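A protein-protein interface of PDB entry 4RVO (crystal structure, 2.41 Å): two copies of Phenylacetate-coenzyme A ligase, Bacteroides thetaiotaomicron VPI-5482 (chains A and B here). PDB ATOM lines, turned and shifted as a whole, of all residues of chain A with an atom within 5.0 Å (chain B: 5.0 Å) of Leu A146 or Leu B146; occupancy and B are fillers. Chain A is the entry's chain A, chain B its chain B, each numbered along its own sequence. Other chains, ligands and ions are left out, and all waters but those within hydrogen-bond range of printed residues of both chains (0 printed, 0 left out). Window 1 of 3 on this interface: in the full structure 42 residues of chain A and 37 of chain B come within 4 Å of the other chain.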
ATOM      1  N   ARG A  90       4.051  15.799  26.998  1.00  0.00           N
ATOM      2  CA  ARG A  90       4.603  17.043  26.441  1.00  0.00           C
ATOM      3  C   ARG A  90       4.899  18.092  27.510  1.00  0.00           C
ATOM      4  O   ARG A  90       4.119  18.268  28.443  1.00  0.00           O
ATOM      5  CB  ARG A  90       3.660  17.648  25.394  1.00  0.00           C
ATOM      6  CG  ARG A  90       4.374  18.660  24.485  1.00  0.00           C
ATOM      7  CD  ARG A  90       3.429  19.392  23.605  1.00  0.00           C
ATOM      8  NE  ARG A  90       2.830  18.524  22.602  1.00  0.00           N
ATOM      9  CZ  ARG A  90       1.840  18.898  21.810  1.00  0.00           C
ATOM     10  NH1 ARG A  90       1.325  20.116  21.913  1.00  0.00           N
ATOM     11  NH2 ARG A  90       1.339  18.054  20.923  1.00  0.00           N
ATOM     12  N   HIS A  92       5.609  22.376  27.721  1.00  0.00           N
ATOM     13  CA  HIS A  92       5.676  23.666  27.091  1.00  0.00           C
ATOM     14  C   HIS A  92       6.320  24.653  28.024  1.00  0.00           C
ATOM     15  O   HIS A  92       5.935  24.744  29.188  1.00  0.00           O
ATOM     16  CB  HIS A  92       4.288  24.146  26.644  1.00  0.00           C
ATOM     17  CG  HIS A  92       3.892  23.620  25.302  1.00  0.00           C
ATOM     18  ND1 HIS A  92       4.535  24.038  24.140  1.00  0.00           N
ATOM     19  CD2 HIS A  92       2.960  22.696  24.976  1.00  0.00           C
ATOM     20  CE1 HIS A  92       3.978  23.354  23.154  1.00  0.00           C
ATOM     21  NE2 HIS A  92       3.011  22.548  23.602  1.00  0.00           N
ATOM     22  N   TRP A 114      -7.313  19.886  24.770  1.00  0.00           N
ATOM     23  CA  TRP A 114      -6.787  21.099  24.173  1.00  0.00           C
ATOM     24  C   TRP A 114      -7.075  21.127  22.663  1.00  0.00           C
ATOM     25  O   TRP A 114      -7.569  22.127  22.155  1.00  0.00           O
ATOM     26  CB  TRP A 114      -5.274  21.196  24.450  1.00  0.00           C
ATOM     27  CG  TRP A 114      -4.578  22.365  23.820  1.00  0.00           C
ATOM     28  CD1 TRP A 114      -5.138  23.556  23.441  1.00  0.00           C
ATOM     29  CD2 TRP A 114      -3.164  22.524  23.675  1.00  0.00           C
ATOM     30  NE1 TRP A 114      -4.166  24.399  22.953  1.00  0.00           N
ATOM     31  CE2 TRP A 114      -2.940  23.794  23.094  1.00  0.00           C
ATOM     32  CE3 TRP A 114      -2.055  21.707  23.967  1.00  0.00           C
ATOM     33  CZ2 TRP A 114      -1.657  24.263  22.796  1.00  0.00           C
ATOM     34  CZ3 TRP A 114      -0.789  22.166  23.653  1.00  0.00           C
ATOM     35  CH2 TRP A 114      -0.597  23.429  23.076  1.00  0.00           C
ATOM     36  N   TYR A 139       6.376  27.361  15.797  1.00  0.00           N
ATOM     37  CA  TYR A 139       6.201  26.034  16.358  1.00  0.00           C
ATOM     38  C   TYR A 139       7.207  25.818  17.502  1.00  0.00           C
ATOM     39  O   TYR A 139       7.554  26.776  18.199  1.00  0.00           O
ATOM     40  CB  TYR A 139       6.330  24.963  15.271  1.00  0.00           C
ATOM     41  CG  TYR A 139       5.063  24.797  14.455  1.00  0.00           C
ATOM     42  CD1 TYR A 139       4.567  25.847  13.677  1.00  0.00           C
ATOM     43  CD2 TYR A 139       4.350  23.604  14.471  1.00  0.00           C
ATOM     44  CE1 TYR A 139       3.369  25.722  12.974  1.00  0.00           C
ATOM     45  CE2 TYR A 139       3.164  23.457  13.749  1.00  0.00           C
ATOM     46  CZ  TYR A 139       2.674  24.523  13.002  1.00  0.00           C
ATOM     47  OH  TYR A 139       1.503  24.391  12.297  1.00  0.00           O
ATOM     48  N   GLY A 140       7.565  24.574  17.759  1.00  0.00           N
ATOM     49  CA  GLY A 140       8.430  24.246  18.882  1.00  0.00           C
ATOM     50  C   GLY A 140       7.737  24.441  20.221  1.00  0.00           C
ATOM     51  O   GLY A 140       6.633  23.925  20.432  1.00  0.00           O
ATOM     52  N   PHE A 142       6.389  27.223  21.347  1.00  0.00           N
ATOM     53  CA  PHE A 142       5.222  28.118  21.220  1.00  0.00           C
ATOM     54  C   PHE A 142       3.943  27.307  21.076  1.00  0.00           C
ATOM     55  O   PHE A 142       3.839  26.470  20.179  1.00  0.00           O
ATOM     56  CB  PHE A 142       5.385  29.064  20.030  1.00  0.00           C
ATOM     57  CG  PHE A 142       6.545  30.015  20.138  1.00  0.00           C
ATOM     58  CD1 PHE A 142       6.438  31.183  20.879  1.00  0.00           C
ATOM     59  CD2 PHE A 142       7.706  29.807  19.401  1.00  0.00           C
ATOM     60  CE1 PHE A 142       7.493  32.094  20.932  1.00  0.00           C
ATOM     61  CE2 PHE A 142       8.756  30.727  19.445  1.00  0.00           C
ATOM     62  CZ  PHE A 142       8.640  31.866  20.203  1.00  0.00           C
ATOM     63  N   THR A 143       2.971  27.543  21.963  1.00  0.00           N
ATOM     64  CA  THR A 143       1.737  26.754  22.014  1.00  0.00           C
ATOM     65  C   THR A 143       0.850  26.992  20.766  1.00  0.00           C
ATOM     66  O   THR A 143       0.012  26.152  20.443  1.00  0.00           O
ATOM     67  CB  THR A 143       0.974  27.061  23.280  1.00  0.00           C
ATOM     68  OG1 THR A 143       0.727  28.465  23.344  1.00  0.00           O
ATOM     69  CG2 THR A 143       1.713  26.605  24.522  1.00  0.00           C
ATOM     70  N   GLY A 144       1.060  28.130  20.080  1.00  0.00           N
ATOM     71  CA  GLY A 144       0.304  28.481  18.875  1.00  0.00           C
ATOM     72  C   GLY A 144       0.545  27.540  17.704  1.00  0.00           C
ATOM     73  O   GLY A 144      -0.352  27.313  16.886  1.00  0.00           O
ATOM     74  N   GLY A 145       1.754  26.977  17.638  1.00  0.00           N
ATOM     75  CA  GLY A 145       2.133  26.055  16.578  1.00  0.00           C
ATOM     76  C   GLY A 145       1.440  24.716  16.683  1.00  0.00           C
ATOM     77  O   GLY A 145       0.538  24.417  15.896  1.00  0.00           O
ATOM     78  N   LEU A 146       1.830  23.905  17.685  1.00  0.00           N
ATOM     79  CA  LEU A 146       1.251  22.573  17.895  1.00  0.00           C
ATOM     80  C   LEU A 146      -0.235  22.657  18.311  1.00  0.00           C
ATOM     81  O   LEU A 146      -1.002  21.740  18.033  1.00  0.00           O
ATOM     82  CB  LEU A 146       2.052  21.803  18.960  1.00  0.00           C
ATOM     83  CG  LEU A 146       3.455  21.327  18.527  1.00  0.00           C
ATOM     84  CD1 LEU A 146       4.262  20.853  19.720  1.00  0.00           C
ATOM     85  CD2 LEU A 146       3.361  20.233  17.478  1.00  0.00           C
ATOM     86  N   GLY A 147      -0.618  23.773  18.944  1.00  0.00           N
ATOM     87  CA  GLY A 147      -1.995  24.008  19.377  1.00  0.00           C
ATOM     88  C   GLY A 147      -2.992  24.028  18.237  1.00  0.00           C
ATOM     89  O   GLY A 147      -3.959  23.257  18.242  1.00  0.00           O
ATOM     90  N   PHE A 148      -2.752  24.886  17.228  1.00  0.00           N
ATOM     91  CA  PHE A 148      -3.623  24.960  16.062  1.00  0.00           C
ATOM     92  C   PHE A 148      -3.403  23.774  15.139  1.00  0.00           C
ATOM     93  O   PHE A 148      -4.336  23.354  14.461  1.00  0.00           O
ATOM     94  CB  PHE A 148      -3.414  26.278  15.296  1.00  0.00           C
ATOM     95  CG  PHE A 148      -4.234  27.417  15.839  1.00  0.00           C
ATOM     96  CD1 PHE A 148      -5.600  27.487  15.599  1.00  0.00           C
ATOM     97  CD2 PHE A 148      -3.651  28.404  16.618  1.00  0.00           C
ATOM     98  CE1 PHE A 148      -6.371  28.513  16.149  1.00  0.00           C
ATOM     99  CE2 PHE A 148      -4.419  29.449  17.139  1.00  0.00           C
ATOM    100  CZ  PHE A 148      -5.772  29.495  16.902  1.00  0.00           C
ATOM    101  N   GLN A 149      -2.166  23.203  15.126  1.00  0.00           N
ATOM    102  CA  GLN A 149      -1.870  22.035  14.292  1.00  0.00           C
ATOM    103  C   GLN A 149      -2.774  20.857  14.681  1.00  0.00           C
ATOM    104  O   GLN A 149      -3.453  20.296  13.823  1.00  0.00           O
ATOM    105  CB  GLN A 149      -0.379  21.637  14.410  1.00  0.00           C
ATOM    106  CG  GLN A 149       0.039  20.507  13.448  1.00  0.00           C
ATOM    107  CD  GLN A 149      -0.088  20.922  11.998  1.00  0.00           C
ATOM    108  OE1 GLN A 149       0.298  22.023  11.607  1.00  0.00           O
ATOM    109  NE2 GLN A 149      -0.616  20.040  11.174  1.00  0.00           N
ATOM    110  N   TYR A 150      -2.842  20.540  15.990  1.00  0.00           N
ATOM    111  CA  TYR A 150      -3.652  19.424  16.489  1.00  0.00           C
ATOM    112  C   TYR A 150      -5.148  19.725  16.353  1.00  0.00           C
ATOM    113  O   TYR A 150      -5.916  18.844  15.976  1.00  0.00           O
ATOM    114  CB  TYR A 150      -3.294  19.110  17.953  1.00  0.00           C
ATOM    115  CG  TYR A 150      -2.043  18.262  18.102  1.00  0.00           C
ATOM    116  CD1 TYR A 150      -0.842  18.642  17.504  1.00  0.00           C
ATOM    117  CD2 TYR A 150      -2.032  17.137  18.920  1.00  0.00           C
ATOM    118  CE1 TYR A 150       0.313  17.878  17.649  1.00  0.00           C
ATOM    119  CE2 TYR A 150      -0.882  16.366  19.075  1.00  0.00           C
ATOM    120  CZ  TYR A 150       0.288  16.733  18.427  1.00  0.00           C
ATOM    121  OH  TYR A 150       1.435  15.992  18.593  1.00  0.00           O
ATOM    122  N   GLY A 151      -5.530  20.983  16.593  1.00  0.00           N
ATOM    123  CA  GLY A 151      -6.915  21.421  16.459  1.00  0.00           C
ATOM    124  C   GLY A 151      -7.435  21.348  15.033  1.00  0.00           C
ATOM    125  O   GLY A 151      -8.519  20.811  14.791  1.00  0.00           O
ATOM    126  N   PRO A 161       1.646  23.580   7.786  1.00  0.00           N
ATOM    127  CA  PRO A 161       2.475  24.045   8.917  1.00  0.00           C
ATOM    128  C   PRO A 161       3.623  24.966   8.446  1.00  0.00           C
ATOM    129  O   PRO A 161       4.793  24.586   8.504  1.00  0.00           O
ATOM    130  CB  PRO A 161       3.001  22.742   9.520  1.00  0.00           C
ATOM    131  CG  PRO A 161       3.049  21.793   8.376  1.00  0.00           C
ATOM    132  CD  PRO A 161       1.915  22.160   7.453  1.00  0.00           C
ATOM    133  N   ARG B  90      -2.606  17.166   5.836  1.00  0.00           N
ATOM    134  CA  ARG B  90      -1.313  17.858   5.967  1.00  0.00           C
ATOM    135  C   ARG B  90      -0.534  17.916   4.655  1.00  0.00           C
ATOM    136  O   ARG B  90      -0.502  16.941   3.907  1.00  0.00           O
ATOM    137  CB  ARG B  90      -0.436  17.203   7.039  1.00  0.00           C
ATOM    138  CG  ARG B  90       0.680  18.132   7.518  1.00  0.00           C
ATOM    139  CD  ARG B  90       1.654  17.441   8.389  1.00  0.00           C
ATOM    140  NE  ARG B  90       1.079  17.078   9.669  1.00  0.00           N
ATOM    141  CZ  ARG B  90       1.707  16.337  10.564  1.00  0.00           C
ATOM    142  NH1 ARG B  90       2.921  15.870  10.312  1.00  0.00           N
ATOM    143  NH2 ARG B  90       1.123  16.040  11.710  1.00  0.00           N
ATOM    144  N   HIS B  92       3.579  18.619   3.473  1.00  0.00           N
ATOM    145  CA  HIS B  92       4.969  18.835   3.876  1.00  0.00           C
ATOM    146  C   HIS B  92       5.839  19.254   2.678  1.00  0.00           C
ATOM    147  O   HIS B  92       5.573  18.845   1.542  1.00  0.00           O
ATOM    148  CB  HIS B  92       5.552  17.591   4.546  1.00  0.00           C
ATOM    149  CG  HIS B  92       5.323  17.546   6.026  1.00  0.00           C
ATOM    150  ND1 HIS B  92       5.992  18.404   6.887  1.00  0.00           N
ATOM    151  CD2 HIS B  92       4.569  16.697   6.758  1.00  0.00           C
ATOM    152  CE1 HIS B  92       5.581  18.085   8.102  1.00  0.00           C
ATOM    153  NE2 HIS B  92       4.736  17.056   8.079  1.00  0.00           N
ATOM    154  N   TRP B 114       2.735   6.801   9.520  1.00  0.00           N
ATOM    155  CA  TRP B 114       4.015   7.480   9.687  1.00  0.00           C
ATOM    156  C   TRP B 114       4.408   7.532  11.187  1.00  0.00           C
ATOM    157  O   TRP B 114       5.486   7.060  11.551  1.00  0.00           O
ATOM    158  CB  TRP B 114       3.927   8.893   9.082  1.00  0.00           C
ATOM    159  CG  TRP B 114       5.139   9.761   9.270  1.00  0.00           C
ATOM    160  CD1 TRP B 114       6.429   9.346   9.464  1.00  0.00           C
ATOM    161  CD2 TRP B 114       5.203  11.176   9.046  1.00  0.00           C
ATOM    162  NE1 TRP B 114       7.280  10.431   9.456  1.00  0.00           N
ATOM    163  CE2 TRP B 114       6.550  11.569   9.216  1.00  0.00           C
ATOM    164  CE3 TRP B 114       4.245  12.159   8.743  1.00  0.00           C
ATOM    165  CZ2 TRP B 114       6.959  12.902   9.110  1.00  0.00           C
ATOM    166  CZ3 TRP B 114       4.656  13.476   8.617  1.00  0.00           C
ATOM    167  CH2 TRP B 114       5.997  13.837   8.795  1.00  0.00           C
ATOM    168  N   TYR B 139      10.984  22.733  13.279  1.00  0.00           N
ATOM    169  CA  TYR B 139       9.536  22.477  13.309  1.00  0.00           C
ATOM    170  C   TYR B 139       8.806  23.386  12.321  1.00  0.00           C
ATOM    171  O   TYR B 139       8.972  24.613  12.363  1.00  0.00           O
ATOM    172  CB  TYR B 139       8.979  22.687  14.727  1.00  0.00           C
ATOM    173  CG  TYR B 139       9.024  21.455  15.601  1.00  0.00           C
ATOM    174  CD1 TYR B 139      10.204  21.067  16.232  1.00  0.00           C
ATOM    175  CD2 TYR B 139       7.856  20.767  15.931  1.00  0.00           C
ATOM    176  CE1 TYR B 139      10.239  19.972  17.093  1.00  0.00           C
ATOM    177  CE2 TYR B 139       7.871  19.701  16.825  1.00  0.00           C
ATOM    178  CZ  TYR B 139       9.067  19.296  17.394  1.00  0.00           C
ATOM    179  OH  TYR B 139       9.089  18.217  18.244  1.00  0.00           O
ATOM    180  N   GLY B 140       7.963  22.785  11.484  1.00  0.00           N
ATOM    181  CA  GLY B 140       7.195  23.511  10.480  1.00  0.00           C
ATOM    182  C   GLY B 140       6.885  22.657   9.272  1.00  0.00           C
ATOM    183  O   GLY B 140       6.221  21.620   9.395  1.00  0.00           O
ATOM    184  N   PHE B 142       9.228  21.085   7.660  1.00  0.00           N
ATOM    185  CA  PHE B 142      10.217  20.008   7.670  1.00  0.00           C
ATOM    186  C   PHE B 142       9.725  18.831   8.498  1.00  0.00           C
ATOM    187  O   PHE B 142       9.284  19.011   9.626  1.00  0.00           O
ATOM    188  CB  PHE B 142      11.568  20.514   8.187  1.00  0.00           C
ATOM    189  CG  PHE B 142      12.135  21.642   7.348  1.00  0.00           C
ATOM    190  CD1 PHE B 142      12.152  21.559   5.954  1.00  0.00           C
ATOM    191  CD2 PHE B 142      12.650  22.786   7.947  1.00  0.00           C
ATOM    192  CE1 PHE B 142      12.624  22.623   5.178  1.00  0.00           C
ATOM    193  CE2 PHE B 142      13.162  23.836   7.168  1.00  0.00           C
ATOM    194  CZ  PHE B 142      13.143  23.747   5.788  1.00  0.00           C
ATOM    195  N   THR B 143       9.824  17.612   7.930  1.00  0.00           N
ATOM    196  CA  THR B 143       9.181  16.407   8.453  1.00  0.00           C
ATOM    197  C   THR B 143       9.829  15.907   9.777  1.00  0.00           C
ATOM    198  O   THR B 143       9.225  15.099  10.488  1.00  0.00           O
ATOM    199  CB  THR B 143       9.215  15.312   7.402  1.00  0.00           C
ATOM    200  OG1 THR B 143      10.572  15.068   7.037  1.00  0.00           O
ATOM    201  CG2 THR B 143       8.397  15.672   6.158  1.00  0.00           C
ATOM    202  N   GLY B 144      11.040  16.366  10.069  1.00  0.00           N
ATOM    203  CA  GLY B 144      11.751  15.961  11.278  1.00  0.00           C
ATOM    204  C   GLY B 144      11.080  16.426  12.558  1.00  0.00           C
ATOM    205  O   GLY B 144      11.136  15.738  13.580  1.00  0.00           O
ATOM    206  N   GLY B 145      10.464  17.609  12.505  1.00  0.00           N
ATOM    207  CA  GLY B 145       9.781  18.193  13.653  1.00  0.00           C
ATOM    208  C   GLY B 145       8.531  17.440  14.039  1.00  0.00           C
ATOM    209  O   GLY B 145       8.530  16.699  15.020  1.00  0.00           O
ATOM    210  N   LEU B 146       7.464  17.584  13.241  1.00  0.00           N
ATOM    211  CA  LEU B 146       6.183  16.923  13.514  1.00  0.00           C
ATOM    212  C   LEU B 146       6.306  15.389  13.433  1.00  0.00           C
ATOM    213  O   LEU B 146       5.570  14.676  14.109  1.00  0.00           O
ATOM    214  CB  LEU B 146       5.099  17.418  12.526  1.00  0.00           C
ATOM    215  CG  LEU B 146       4.576  18.857  12.761  1.00  0.00           C
ATOM    216  CD1 LEU B 146       3.732  19.316  11.613  1.00  0.00           C
ATOM    217  CD2 LEU B 146       3.786  18.946  14.035  1.00  0.00           C
ATOM    218  N   GLY B 147       7.234  14.909  12.602  1.00  0.00           N
ATOM    219  CA  GLY B 147       7.457  13.478  12.400  1.00  0.00           C
ATOM    220  C   GLY B 147       7.910  12.757  13.642  1.00  0.00           C
ATOM    221  O   GLY B 147       7.365  11.706  13.982  1.00  0.00           O
ATOM    222  N   PHE B 148       8.909  13.324  14.352  1.00  0.00           N
ATOM    223  CA  PHE B 148       9.385  12.741  15.613  1.00  0.00           C
ATOM    224  C   PHE B 148       8.461  13.113  16.787  1.00  0.00           C
ATOM    225  O   PHE B 148       8.385  12.370  17.758  1.00  0.00           O
ATOM    226  CB  PHE B 148      10.818  13.171  15.907  1.00  0.00           C
ATOM    227  CG  PHE B 148      11.854  12.248  15.314  1.00  0.00           C
ATOM    228  CD1 PHE B 148      12.099  10.998  15.873  1.00  0.00           C
ATOM    229  CD2 PHE B 148      12.602  12.634  14.210  1.00  0.00           C
ATOM    230  CE1 PHE B 148      13.038  10.136  15.308  1.00  0.00           C
ATOM    231  CE2 PHE B 148      13.563  11.781  13.667  1.00  0.00           C
ATOM    232  CZ  PHE B 148      13.770  10.535  14.215  1.00  0.00           C
ATOM    233  N   GLN B 149       7.752  14.252  16.684  1.00  0.00           N
ATOM    234  CA  GLN B 149       6.808  14.691  17.717  1.00  0.00           C
ATOM    235  C   GLN B 149       5.656  13.688  17.852  1.00  0.00           C
ATOM    236  O   GLN B 149       5.371  13.221  18.953  1.00  0.00           O
ATOM    237  CB  GLN B 149       6.261  16.109  17.383  1.00  0.00           C
ATOM    238  CG  GLN B 149       5.373  16.715  18.488  1.00  0.00           C
ATOM    239  CD  GLN B 149       6.139  16.923  19.785  1.00  0.00           C
ATOM    240  OE1 GLN B 149       7.286  17.385  19.797  1.00  0.00           O
ATOM    241  NE2 GLN B 149       5.510  16.615  20.895  1.00  0.00           N
ATOM    242  N   TYR B 150       5.041  13.308  16.724  1.00  0.00           N
ATOM    243  CA  TYR B 150       3.920  12.363  16.712  1.00  0.00           C
ATOM    244  C   TYR B 150       4.372  10.959  17.115  1.00  0.00           C
ATOM    245  O   TYR B 150       3.670  10.283  17.858  1.00  0.00           O
ATOM    246  CB  TYR B 150       3.258  12.333  15.325  1.00  0.00           C
ATOM    247  CG  TYR B 150       2.279  13.469  15.100  1.00  0.00           C
ATOM    248  CD1 TYR B 150       2.655  14.794  15.315  1.00  0.00           C
ATOM    249  CD2 TYR B 150       1.012  13.229  14.570  1.00  0.00           C
ATOM    250  CE1 TYR B 150       1.763  15.843  15.101  1.00  0.00           C
ATOM    251  CE2 TYR B 150       0.114  14.272  14.343  1.00  0.00           C
ATOM    252  CZ  TYR B 150       0.488  15.578  14.626  1.00  0.00           C
ATOM    253  OH  TYR B 150      -0.379  16.610  14.379  1.00  0.00           O
ATOM    254  N   GLY B 151       5.560  10.555  16.660  1.00  0.00           N
ATOM    255  CA  GLY B 151       6.127   9.253  17.000  1.00  0.00           C
ATOM    256  C   GLY B 151       6.415   9.096  18.481  1.00  0.00           C
ATOM    257  O   GLY B 151       5.992   8.111  19.101  1.00  0.00           O
ATOM    258  N   PRO B 161       9.538  19.687  22.729  1.00  0.00           N
ATOM    259  CA  PRO B 161       9.648  20.216  21.347  1.00  0.00           C
ATOM    260  C   PRO B 161      10.535  21.465  21.291  1.00  0.00           C
ATOM    261  O   PRO B 161      10.040  22.569  21.054  1.00  0.00           O
ATOM    262  CB  PRO B 161       8.198  20.531  20.978  1.00  0.00           C
ATOM    263  CG  PRO B 161       7.536  20.845  22.284  1.00  0.00           C
ATOM    264  CD  PRO B 161       8.214  19.984  23.329  1.00  0.00           C
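Arg A90 touches Gln B149, and with the chains exchanged Gln A149 touches Arg B90. Tyr A139 touches its own counterpart, Tyr B139. Gly A140 touches Tyr B139, but with the chains exchanged Tyr A139 does not touch Gly B140 (4.6 Å). Gly A140 touches Pro B161, and with the chains exchanged Pro A161 touches Gly B140. 16 positions are printed for both chains.
The guanidinium group of Arg B90 sits close to the side-chain hydroxyl of Tyr B150 (3.1 Å). NE2 of His B92 is in hydrogen-bond range of NH1 of Arg B90 (3.1 Å). The side-chain amide oxygen (OE1) of Gln B149 sits at hydrogen-bond distance from the side-chain hydroxyl (OH) of Tyr B139 (2.5 Å). The guanidinium group (NH2) of Arg A90 sits close to the side-chain hydroxyl (OH) of Tyr A150 (3.1 Å). The guanidinium group (NH1) of Arg A90 sits close to a ring nitrogen (NE2) of His A92, 3.4 Å away. The side-chain hydroxyl (OH) of Tyr A139 is in hydrogen-bond range of the side-chain amide oxygen (OE1) of Gln A149 (2.7 Å).
O of Pro A161 lies close to O of Gly B140 (3.4 Å).
Of the printed residues of chain B, Arg A90 touches Gln B149 (3.7 Å). Of the printed residues of chain B, Tyr A139 touches Tyr B139. Leu A146 touches just one residue of chain B: Leu B146 (3.7 Å). Printed residues of chain B within 4 Å of Gln A149: Arg B90 (3.7 Å). Of the printed residues of chain B, Pro A161 touches Gly B140 (2.9 Å). Of chain A, only Leu A146 (3.7 Å) comes within 4 Å of Leu B146. Printed residues of chain A within 4 Å of Tyr B150: Tyr A150. The nearest printed residue of chain A that does not touch Leu B146 is Pro A161 (4.1 Å).
Gln B149 touches Arg A90 (NE2 to NE, 3.7 Å). Tyr B139 touches Tyr A139. Gly A140 touches Tyr B139 (N to CB, 3.8 Å). Pro B161 touches Gly A140. Leu A146 touches Leu B146 (CD2 to CD2, 3.7 Å). Gln A149 touches Arg B90 (NE2 to NE, 3.7 Å). CE1 of Tyr B150 touches OH of Tyr A150 (3.5 Å).
Of the 16 printed residues of chain A, 7 touch a printed residue of chain B. Printed residues of chain A that touch a printed residue of chain B: Arg A90, Tyr A139, Gly A140, Leu A146, Gln A149, Tyr A150 and Pro A161. Hydrophobic or aromatic side chains of chain A within 4 Å of the printed part of chain B: Tyr A139, Leu A146, Tyr A150 and Pro A161. Hydrophobic or aromatic side chains of chain B within 4 Å of the printed part of chain A: Tyr B139, Leu B146, Tyr B150 and Pro B161.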
